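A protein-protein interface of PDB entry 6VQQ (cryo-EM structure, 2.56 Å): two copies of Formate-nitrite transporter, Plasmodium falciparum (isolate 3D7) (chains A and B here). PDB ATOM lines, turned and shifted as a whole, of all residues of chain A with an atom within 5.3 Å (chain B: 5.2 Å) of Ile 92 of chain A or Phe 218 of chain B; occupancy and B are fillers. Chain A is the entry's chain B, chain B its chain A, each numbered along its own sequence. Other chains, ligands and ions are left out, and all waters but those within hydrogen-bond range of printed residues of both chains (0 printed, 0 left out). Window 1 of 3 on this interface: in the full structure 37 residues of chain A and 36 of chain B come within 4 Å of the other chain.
Printed residues of chain B that touch a printed residue of chain A: Phe 195, Phe 202, Phe 214, Ser 215, Phe 218 and Tyr 221. Hydrophobic or aromatic side chains of chain B within 4 Å of the printed part of chain A: Phe 195, Phe 202, Phe 214, Phe 218 and Tyr 221. Of the 13 printed residues of chain A, 8 touch a printed residue of chain B. Hydrophobic or aromatic side chains of chain A that line the printed part of chain B: Phe 88, Ile 92, Met 95, Val 213 and Phe 214. Among the printed residues, 11 pairs touch across the chains. Among the printed residues, no Asp or Glu carboxylate lies within 4 Å of a Lys or Arg side-chain nitrogen of the other chain.
The side-chain hydroxyl of Tyr 221 of chain B lies within hydrogen-bond range of the side-chain hydroxyl of Thr 89 of chain A (3.5 Å).
Phe 214 of chain A touches its own counterpart, Phe 214 of chain B. Positions printed for both chains: 214 and 217.
CZ of Phe 195 of chain B touches SG of Cys 57 of chain A, 3.9 Å away. Phe 88 of chain A touches Phe 218 of chain B (CE1 to CE1, 3.7 Å). Tyr 221 of chain B touches Phe 88 of chain A (CE2 to CD2, 3.9 Å). Phe 195 of chain B touches Ile 92 of chain A (CE1 to CG2, 3.9 Å). Phe 218 of chain B touches Ile 92 of chain A (CB to CD1, 3.8 Å). Met 95 of chain A touches Phe 202 of chain B. N of Cys 96 of chain A touches CZ of Phe 202 of chain B, 3.6 Å away. Ser 215 of chain B touches Val 213 of chain A. Val 213 of chain A touches Phe 218 of chain B. CZ of Phe 214 of chain A touches CD2 of Phe 214 of chain B, 3.3 Å away.
Ile 92 of chain A touches just these residues of chain B: Phe 195 (3.9 Å) and Phe 218 (3.8 Å). Of chain A, only Phe 88 (3.7 Å), Ile 92 (3.8 Å) and Val 213 (3.6 Å) come within 4 Å of Phe 218 of chain B. Of the printed residues of chain B, Phe 214 of chain A touches Phe 214 (3.3 Å). Of the printed residues of chain A, Ser 215 of chain B touches Val 213 (3.5 Å). Ala 222 of chain B touches none of the printed residues of chain A. The nearest residue of chain B that does not touch Ile 92 of chain A is Phe 202 of chain B (4.02 Å). The nearest residue of chain A that does not touch Phe 218 of chain B is Phe 217 of chain A (4.04 Å). The nearest printed residue of chain B that does not touch Val 213 of chain A is Phe 214 of chain B (4.4 Å).
The side-chain sulfur (SG) of Cys 57 of chain A is in hydrogen-bond range of the backbone NH (N) of Ala 93 of chain A. O of Ile 92 of chain A lies within hydrogen-bond range of SG of Cys 96 of chain A (2.9 Å).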
ATOM      1  N   CYS A  57      -6.260  29.724  -7.104  1.00  0.00           N
ATOM      2  CA  CYS A  57      -6.287  28.611  -8.040  1.00  0.00           C
ATOM      3  C   CYS A  57      -5.215  27.581  -7.714  1.00  0.00           C
ATOM      4  O   CYS A  57      -5.432  26.380  -7.915  1.00  0.00           O
ATOM      5  CB  CYS A  57      -6.135  29.136  -9.462  1.00  0.00           C
ATOM      6  SG  CYS A  57      -7.480  30.222  -9.979  1.00  0.00           S
ATOM      7  N   PHE A  88      -5.673  20.623 -15.144  1.00  0.00           N
ATOM      8  CA  PHE A  88      -7.062  20.837 -15.531  1.00  0.00           C
ATOM      9  C   PHE A  88      -7.706  21.932 -14.690  1.00  0.00           C
ATOM     10  O   PHE A  88      -8.631  22.613 -15.146  1.00  0.00           O
ATOM     11  CB  PHE A  88      -7.842  19.532 -15.397  1.00  0.00           C
ATOM     12  CG  PHE A  88      -9.278  19.629 -15.827  1.00  0.00           C
ATOM     13  CD1 PHE A  88      -9.610  20.128 -17.073  1.00  0.00           C
ATOM     14  CD2 PHE A  88     -10.296  19.209 -14.988  1.00  0.00           C
ATOM     15  CE1 PHE A  88     -10.929  20.215 -17.470  1.00  0.00           C
ATOM     16  CE2 PHE A  88     -11.612  19.292 -15.379  1.00  0.00           C
ATOM     17  CZ  PHE A  88     -11.931  19.796 -16.622  1.00  0.00           C
ATOM     18  N   THR A  89      -7.224  22.117 -13.463  1.00  0.00           N
ATOM     19  CA  THR A  89      -7.861  23.042 -12.531  1.00  0.00           C
ATOM     20  C   THR A  89      -7.232  24.429 -12.578  1.00  0.00           C
ATOM     21  O   THR A  89      -7.937  25.437 -12.455  1.00  0.00           O
ATOM     22  CB  THR A  89      -7.781  22.475 -11.114  1.00  0.00           C
ATOM     23  OG1 THR A  89      -8.188  21.104 -11.123  1.00  0.00           O
ATOM     24  CG2 THR A  89      -8.663  23.251 -10.176  1.00  0.00           C
ATOM     25  N   PHE A  90      -5.916  24.504 -12.758  1.00  0.00           N
ATOM     26  CA  PHE A  90      -5.233  25.790 -12.664  1.00  0.00           C
ATOM     27  C   PHE A  90      -5.692  26.800 -13.708  1.00  0.00           C
ATOM     28  O   PHE A  90      -5.839  27.984 -13.356  1.00  0.00           O
ATOM     29  CB  PHE A  90      -3.721  25.559 -12.761  1.00  0.00           C
ATOM     30  CG  PHE A  90      -2.889  26.765 -12.417  1.00  0.00           C
ATOM     31  CD1 PHE A  90      -2.752  27.811 -13.309  1.00  0.00           C
ATOM     32  CD2 PHE A  90      -2.228  26.840 -11.206  1.00  0.00           C
ATOM     33  CE1 PHE A  90      -1.985  28.907 -12.996  1.00  0.00           C
ATOM     34  CE2 PHE A  90      -1.460  27.936 -10.889  1.00  0.00           C
ATOM     35  CZ  PHE A  90      -1.338  28.971 -11.784  1.00  0.00           C
ATOM     36  N   PRO A  91      -5.930  26.436 -14.968  1.00  0.00           N
ATOM     37  CA  PRO A  91      -6.259  27.458 -15.973  1.00  0.00           C
ATOM     38  C   PRO A  91      -7.613  28.120 -15.775  1.00  0.00           C
ATOM     39  O   PRO A  91      -8.486  28.057 -16.645  1.00  0.00           O
ATOM     40  CB  PRO A  91      -6.216  26.678 -17.296  1.00  0.00           C
ATOM     41  CG  PRO A  91      -6.147  25.256 -16.937  1.00  0.00           C
ATOM     42  CD  PRO A  91      -5.557  25.159 -15.593  1.00  0.00           C
ATOM     43  N   ILE A  92      -7.797  28.761 -14.624  1.00  0.00           N
ATOM     44  CA  ILE A  92      -8.906  29.690 -14.439  1.00  0.00           C
ATOM     45  C   ILE A  92      -8.470  30.999 -13.810  1.00  0.00           C
ATOM     46  O   ILE A  92      -9.213  31.993 -13.882  1.00  0.00           O
ATOM     47  CB  ILE A  92     -10.031  29.034 -13.605  1.00  0.00           C
ATOM     48  CG1 ILE A  92     -11.295  29.896 -13.603  1.00  0.00           C
ATOM     49  CG2 ILE A  92      -9.574  28.795 -12.193  1.00  0.00           C
ATOM     50  CD1 ILE A  92     -11.907  30.108 -14.962  1.00  0.00           C
ATOM     51  N   ALA A  93      -7.278  31.062 -13.216  1.00  0.00           N
ATOM     52  CA  ALA A  93      -6.720  32.330 -12.767  1.00  0.00           C
ATOM     53  C   ALA A  93      -6.536  33.299 -13.920  1.00  0.00           C
ATOM     54  O   ALA A  93      -6.757  34.507 -13.768  1.00  0.00           O
ATOM     55  CB  ALA A  93      -5.381  32.081 -12.085  1.00  0.00           C
ATOM     56  N   PHE A  94      -6.119  32.789 -15.077  1.00  0.00           N
ATOM     57  CA  PHE A  94      -5.821  33.649 -16.210  1.00  0.00           C
ATOM     58  C   PHE A  94      -7.062  34.395 -16.682  1.00  0.00           C
ATOM     59  O   PHE A  94      -6.994  35.590 -16.987  1.00  0.00           O
ATOM     60  CB  PHE A  94      -5.226  32.809 -17.334  1.00  0.00           C
ATOM     61  CG  PHE A  94      -4.496  33.609 -18.365  1.00  0.00           C
ATOM     62  CD1 PHE A  94      -3.217  34.074 -18.119  1.00  0.00           C
ATOM     63  CD2 PHE A  94      -5.088  33.899 -19.581  1.00  0.00           C
ATOM     64  CE1 PHE A  94      -2.543  34.811 -19.067  1.00  0.00           C
ATOM     65  CE2 PHE A  94      -4.420  34.635 -20.530  1.00  0.00           C
ATOM     66  CZ  PHE A  94      -3.148  35.092 -20.274  1.00  0.00           C
ATOM     67  N   MET A  95      -8.206  33.712 -16.740  1.00  0.00           N
ATOM     68  CA  MET A  95      -9.432  34.374 -17.171  1.00  0.00           C
ATOM     69  C   MET A  95      -9.853  35.434 -16.165  1.00  0.00           C
ATOM     70  O   MET A  95     -10.287  36.528 -16.541  1.00  0.00           O
ATOM     71  CB  MET A  95     -10.542  33.345 -17.366  1.00  0.00           C
ATOM     72  CG  MET A  95     -10.368  32.442 -18.581  1.00  0.00           C
ATOM     73  SD  MET A  95     -10.038  33.312 -20.129  1.00  0.00           S
ATOM     74  CE  MET A  95     -11.276  34.606 -20.085  1.00  0.00           C
ATOM     75  N   CYS A  96      -9.772  35.108 -14.877  1.00  0.00           N
ATOM     76  CA  CYS A  96      -9.962  36.103 -13.830  1.00  0.00           C
ATOM     77  C   CYS A  96      -9.150  37.360 -14.109  1.00  0.00           C
ATOM     78  O   CYS A  96      -9.695  38.465 -14.221  1.00  0.00           O
ATOM     79  CB  CYS A  96      -9.564  35.505 -12.482  1.00  0.00           C
ATOM     80  SG  CYS A  96     -10.388  33.955 -12.070  1.00  0.00           S
ATOM     81  N   VAL A 213     -11.237  31.137 -23.365  1.00  0.00           N
ATOM     82  CA  VAL A 213     -11.254  30.095 -22.349  1.00  0.00           C
ATOM     83  C   VAL A 213     -10.416  28.906 -22.786  1.00  0.00           C
ATOM     84  O   VAL A 213      -9.510  28.476 -22.067  1.00  0.00           O
ATOM     85  CB  VAL A 213     -12.705  29.680 -22.042  1.00  0.00           C
ATOM     86  CG1 VAL A 213     -12.748  28.581 -20.983  1.00  0.00           C
ATOM     87  CG2 VAL A 213     -13.520  30.880 -21.595  1.00  0.00           C
ATOM     88  N   PHE A 214     -10.676  28.370 -23.977  1.00  0.00           N
ATOM     89  CA  PHE A 214     -10.078  27.089 -24.323  1.00  0.00           C
ATOM     90  C   PHE A 214      -8.637  27.241 -24.793  1.00  0.00           C
ATOM     91  O   PHE A 214      -7.793  26.390 -24.485  1.00  0.00           O
ATOM     92  CB  PHE A 214     -10.937  26.390 -25.371  1.00  0.00           C
ATOM     93  CG  PHE A 214     -12.239  25.895 -24.828  1.00  0.00           C
ATOM     94  CD1 PHE A 214     -12.275  24.811 -23.973  1.00  0.00           C
ATOM     95  CD2 PHE A 214     -13.424  26.523 -25.154  1.00  0.00           C
ATOM     96  CE1 PHE A 214     -13.470  24.354 -23.462  1.00  0.00           C
ATOM     97  CE2 PHE A 214     -14.624  26.071 -24.646  1.00  0.00           C
ATOM     98  CZ  PHE A 214     -14.646  24.986 -23.800  1.00  0.00           C
ATOM     99  N   PHE A 217      -6.796  27.637 -21.652  1.00  0.00           N
ATOM    100  CA  PHE A 217      -6.850  26.388 -20.907  1.00  0.00           C
ATOM    101  C   PHE A 217      -5.804  25.413 -21.415  1.00  0.00           C
ATOM    102  O   PHE A 217      -5.030  24.855 -20.633  1.00  0.00           O
ATOM    103  CB  PHE A 217      -8.242  25.763 -21.003  1.00  0.00           C
ATOM    104  CG  PHE A 217      -8.271  24.325 -20.591  1.00  0.00           C
ATOM    105  CD1 PHE A 217      -8.254  23.975 -19.256  1.00  0.00           C
ATOM    106  CD2 PHE A 217      -8.284  23.324 -21.538  1.00  0.00           C
ATOM    107  CE1 PHE A 217      -8.265  22.655 -18.875  1.00  0.00           C
ATOM    108  CE2 PHE A 217      -8.295  22.000 -21.161  1.00  0.00           C
ATOM    109  CZ  PHE A 217      -8.284  21.667 -19.827  1.00  0.00           C
ATOM    110  N   PHE B 195     -14.672  32.887  -5.980  1.00  0.00           N
ATOM    111  CA  PHE B 195     -14.930  32.211  -7.251  1.00  0.00           C
ATOM    112  C   PHE B 195     -16.328  32.518  -7.779  1.00  0.00           C
ATOM    113  O   PHE B 195     -16.517  32.726  -8.984  1.00  0.00           O
ATOM    114  CB  PHE B 195     -14.747  30.701  -7.099  1.00  0.00           C
ATOM    115  CG  PHE B 195     -13.386  30.204  -7.506  1.00  0.00           C
ATOM    116  CD1 PHE B 195     -12.857  30.517  -8.742  1.00  0.00           C
ATOM    117  CD2 PHE B 195     -12.647  29.402  -6.657  1.00  0.00           C
ATOM    118  CE1 PHE B 195     -11.615  30.054  -9.115  1.00  0.00           C
ATOM    119  CE2 PHE B 195     -11.405  28.935  -7.030  1.00  0.00           C
ATOM    120  CZ  PHE B 195     -10.890  29.262  -8.255  1.00  0.00           C
ATOM    121  N   PHE B 202     -17.864  37.228 -14.943  1.00  0.00           N
ATOM    122  CA  PHE B 202     -17.720  36.598 -16.252  1.00  0.00           C
ATOM    123  C   PHE B 202     -19.006  36.703 -17.058  1.00  0.00           C
ATOM    124  O   PHE B 202     -19.049  37.343 -18.115  1.00  0.00           O
ATOM    125  CB  PHE B 202     -17.337  35.121 -16.088  1.00  0.00           C
ATOM    126  CG  PHE B 202     -15.886  34.874 -15.791  1.00  0.00           C
ATOM    127  CD1 PHE B 202     -14.910  35.803 -16.101  1.00  0.00           C
ATOM    128  CD2 PHE B 202     -15.504  33.682 -15.207  1.00  0.00           C
ATOM    129  CE1 PHE B 202     -13.591  35.549 -15.829  1.00  0.00           C
ATOM    130  CE2 PHE B 202     -14.186  33.424 -14.934  1.00  0.00           C
ATOM    131  CZ  PHE B 202     -13.227  34.355 -15.246  1.00  0.00           C
ATOM    132  N   PHE B 214     -18.889  27.833 -19.999  1.00  0.00           N
ATOM    133  CA  PHE B 214     -17.635  27.225 -19.572  1.00  0.00           C
ATOM    134  C   PHE B 214     -16.868  28.093 -18.583  1.00  0.00           C
ATOM    135  O   PHE B 214     -16.207  27.560 -17.678  1.00  0.00           O
ATOM    136  CB  PHE B 214     -16.779  26.922 -20.798  1.00  0.00           C
ATOM    137  CG  PHE B 214     -17.139  25.633 -21.471  1.00  0.00           C
ATOM    138  CD1 PHE B 214     -16.889  24.420 -20.856  1.00  0.00           C
ATOM    139  CD2 PHE B 214     -17.747  25.634 -22.712  1.00  0.00           C
ATOM    140  CE1 PHE B 214     -17.226  23.236 -21.469  1.00  0.00           C
ATOM    141  CE2 PHE B 214     -18.084  24.451 -23.330  1.00  0.00           C
ATOM    142  CZ  PHE B 214     -17.823  23.250 -22.707  1.00  0.00           C
ATOM    143  N   SER B 215     -16.934  29.417 -18.732  1.00  0.00           N
ATOM    144  CA  SER B 215     -16.325  30.295 -17.744  1.00  0.00           C
ATOM    145  C   SER B 215     -16.900  30.030 -16.362  1.00  0.00           C
ATOM    146  O   SER B 215     -16.208  30.183 -15.348  1.00  0.00           O
ATOM    147  CB  SER B 215     -16.544  31.752 -18.146  1.00  0.00           C
ATOM    148  OG  SER B 215     -15.595  32.157 -19.113  1.00  0.00           O
ATOM    149  N   VAL B 216     -18.167  29.627 -16.305  1.00  0.00           N
ATOM    150  CA  VAL B 216     -18.787  29.307 -15.029  1.00  0.00           C
ATOM    151  C   VAL B 216     -18.503  27.863 -14.648  1.00  0.00           C
ATOM    152  O   VAL B 216     -18.298  27.558 -13.468  1.00  0.00           O
ATOM    153  CB  VAL B 216     -20.297  29.579 -15.096  1.00  0.00           C
ATOM    154  CG1 VAL B 216     -20.960  29.261 -13.769  1.00  0.00           C
ATOM    155  CG2 VAL B 216     -20.560  31.011 -15.503  1.00  0.00           C
ATOM    156  N   PHE B 217     -18.502  26.957 -15.627  1.00  0.00           N
ATOM    157  CA  PHE B 217     -18.161  25.566 -15.362  1.00  0.00           C
ATOM    158  C   PHE B 217     -16.846  25.460 -14.608  1.00  0.00           C
ATOM    159  O   PHE B 217     -16.758  24.786 -13.578  1.00  0.00           O
ATOM    160  CB  PHE B 217     -18.082  24.783 -16.674  1.00  0.00           C
ATOM    161  CG  PHE B 217     -17.413  23.454 -16.537  1.00  0.00           C
ATOM    162  CD1 PHE B 217     -18.143  22.333 -16.208  1.00  0.00           C
ATOM    163  CD2 PHE B 217     -16.049  23.327 -16.721  1.00  0.00           C
ATOM    164  CE1 PHE B 217     -17.532  21.112 -16.071  1.00  0.00           C
ATOM    165  CE2 PHE B 217     -15.431  22.106 -16.584  1.00  0.00           C
ATOM    166  CZ  PHE B 217     -16.174  20.997 -16.258  1.00  0.00           C
ATOM    167  N   PHE B 218     -15.802  26.103 -15.128  1.00  0.00           N
ATOM    168  CA  PHE B 218     -14.477  25.943 -14.537  1.00  0.00           C
ATOM    169  C   PHE B 218     -14.429  26.511 -13.126  1.00  0.00           C
ATOM    170  O   PHE B 218     -13.917  25.866 -12.206  1.00  0.00           O
ATOM    171  CB  PHE B 218     -13.423  26.612 -15.419  1.00  0.00           C
ATOM    172  CG  PHE B 218     -13.014  25.789 -16.612  1.00  0.00           C
ATOM    173  CD1 PHE B 218     -12.635  24.465 -16.466  1.00  0.00           C
ATOM    174  CD2 PHE B 218     -13.003  26.344 -17.877  1.00  0.00           C
ATOM    175  CE1 PHE B 218     -12.260  23.712 -17.557  1.00  0.00           C
ATOM    176  CE2 PHE B 218     -12.628  25.595 -18.974  1.00  0.00           C
ATOM    177  CZ  PHE B 218     -12.255  24.277 -18.813  1.00  0.00           C
ATOM    178  N   ALA B 219     -14.965  27.716 -12.936  1.00  0.00           N
ATOM    179  CA  ALA B 219     -14.951  28.336 -11.615  1.00  0.00           C
ATOM    180  C   ALA B 219     -15.704  27.488 -10.600  1.00  0.00           C
ATOM    181  O   ALA B 219     -15.259  27.324  -9.453  1.00  0.00           O
ATOM    182  CB  ALA B 219     -15.554  29.735 -11.702  1.00  0.00           C
ATOM    183  N   VAL B 220     -16.862  26.955 -10.994  1.00  0.00           N
ATOM    184  CA  VAL B 220     -17.643  26.160 -10.059  1.00  0.00           C
ATOM    185  C   VAL B 220     -16.939  24.848  -9.752  1.00  0.00           C
ATOM    186  O   VAL B 220     -16.842  24.444  -8.587  1.00  0.00           O
ATOM    187  CB  VAL B 220     -19.064  25.924 -10.591  1.00  0.00           C
ATOM    188  CG1 VAL B 220     -19.851  25.115  -9.578  1.00  0.00           C
ATOM    189  CG2 VAL B 220     -19.763  27.246 -10.874  1.00  0.00           C
ATOM    190  N   TYR B 221     -16.453  24.152 -10.782  1.00  0.00           N
ATOM    191  CA  TYR B 221     -15.659  22.956 -10.535  1.00  0.00           C
ATOM    192  C   TYR B 221     -14.535  23.257  -9.557  1.00  0.00           C
ATOM    193  O   TYR B 221     -14.230  22.445  -8.675  1.00  0.00           O
ATOM    194  CB  TYR B 221     -15.091  22.416 -11.846  1.00  0.00           C
ATOM    195  CG  TYR B 221     -13.948  21.458 -11.629  1.00  0.00           C
ATOM    196  CD1 TYR B 221     -14.163  20.222 -11.043  1.00  0.00           C
ATOM    197  CD2 TYR B 221     -12.652  21.800 -11.980  1.00  0.00           C
ATOM    198  CE1 TYR B 221     -13.129  19.349 -10.827  1.00  0.00           C
ATOM    199  CE2 TYR B 221     -11.610  20.935 -11.766  1.00  0.00           C
ATOM    200  CZ  TYR B 221     -11.850  19.710 -11.189  1.00  0.00           C
ATOM    201  OH  TYR B 221     -10.807  18.841 -10.974  1.00  0.00           O
ATOM    202  N   ALA B 222     -13.936  24.441  -9.678  1.00  0.00           N
ATOM    203  CA  ALA B 222     -12.794  24.779  -8.844  1.00  0.00           C
ATOM    204  C   ALA B 222     -13.202  24.942  -7.390  1.00  0.00           C
ATOM    205  O   ALA B 222     -12.656  24.264  -6.509  1.00  0.00           O
ATOM    206  CB  ALA B 222     -12.136  26.053  -9.362  1.00  0.00           C
ATOM    207  N   PHE B 223     -14.156  25.836  -7.107  1.00  0.00           N
ATOM    208  CA  PHE B 223     -14.481  26.031  -5.697  1.00  0.00           C
ATOM    209  C   PHE B 223     -15.199  24.822  -5.120  1.00  0.00           C
ATOM    210  O   PHE B 223     -15.334  24.715  -3.896  1.00  0.00           O
ATOM    211  CB  PHE B 223     -15.298  27.308  -5.436  1.00  0.00           C
ATOM    212  CG  PHE B 223     -16.748  27.253  -5.844  1.00  0.00           C
ATOM    213  CD1 PHE B 223     -17.678  26.548  -5.091  1.00  0.00           C
ATOM    214  CD2 PHE B 223     -17.189  27.939  -6.955  1.00  0.00           C
ATOM    215  CE1 PHE B 223     -19.003  26.520  -5.455  1.00  0.00           C
ATOM    216  CE2 PHE B 223     -18.523  27.924  -7.307  1.00  0.00           C
ATOM    217  CZ  PHE B 223     -19.423  27.204  -6.565  1.00  0.00           C
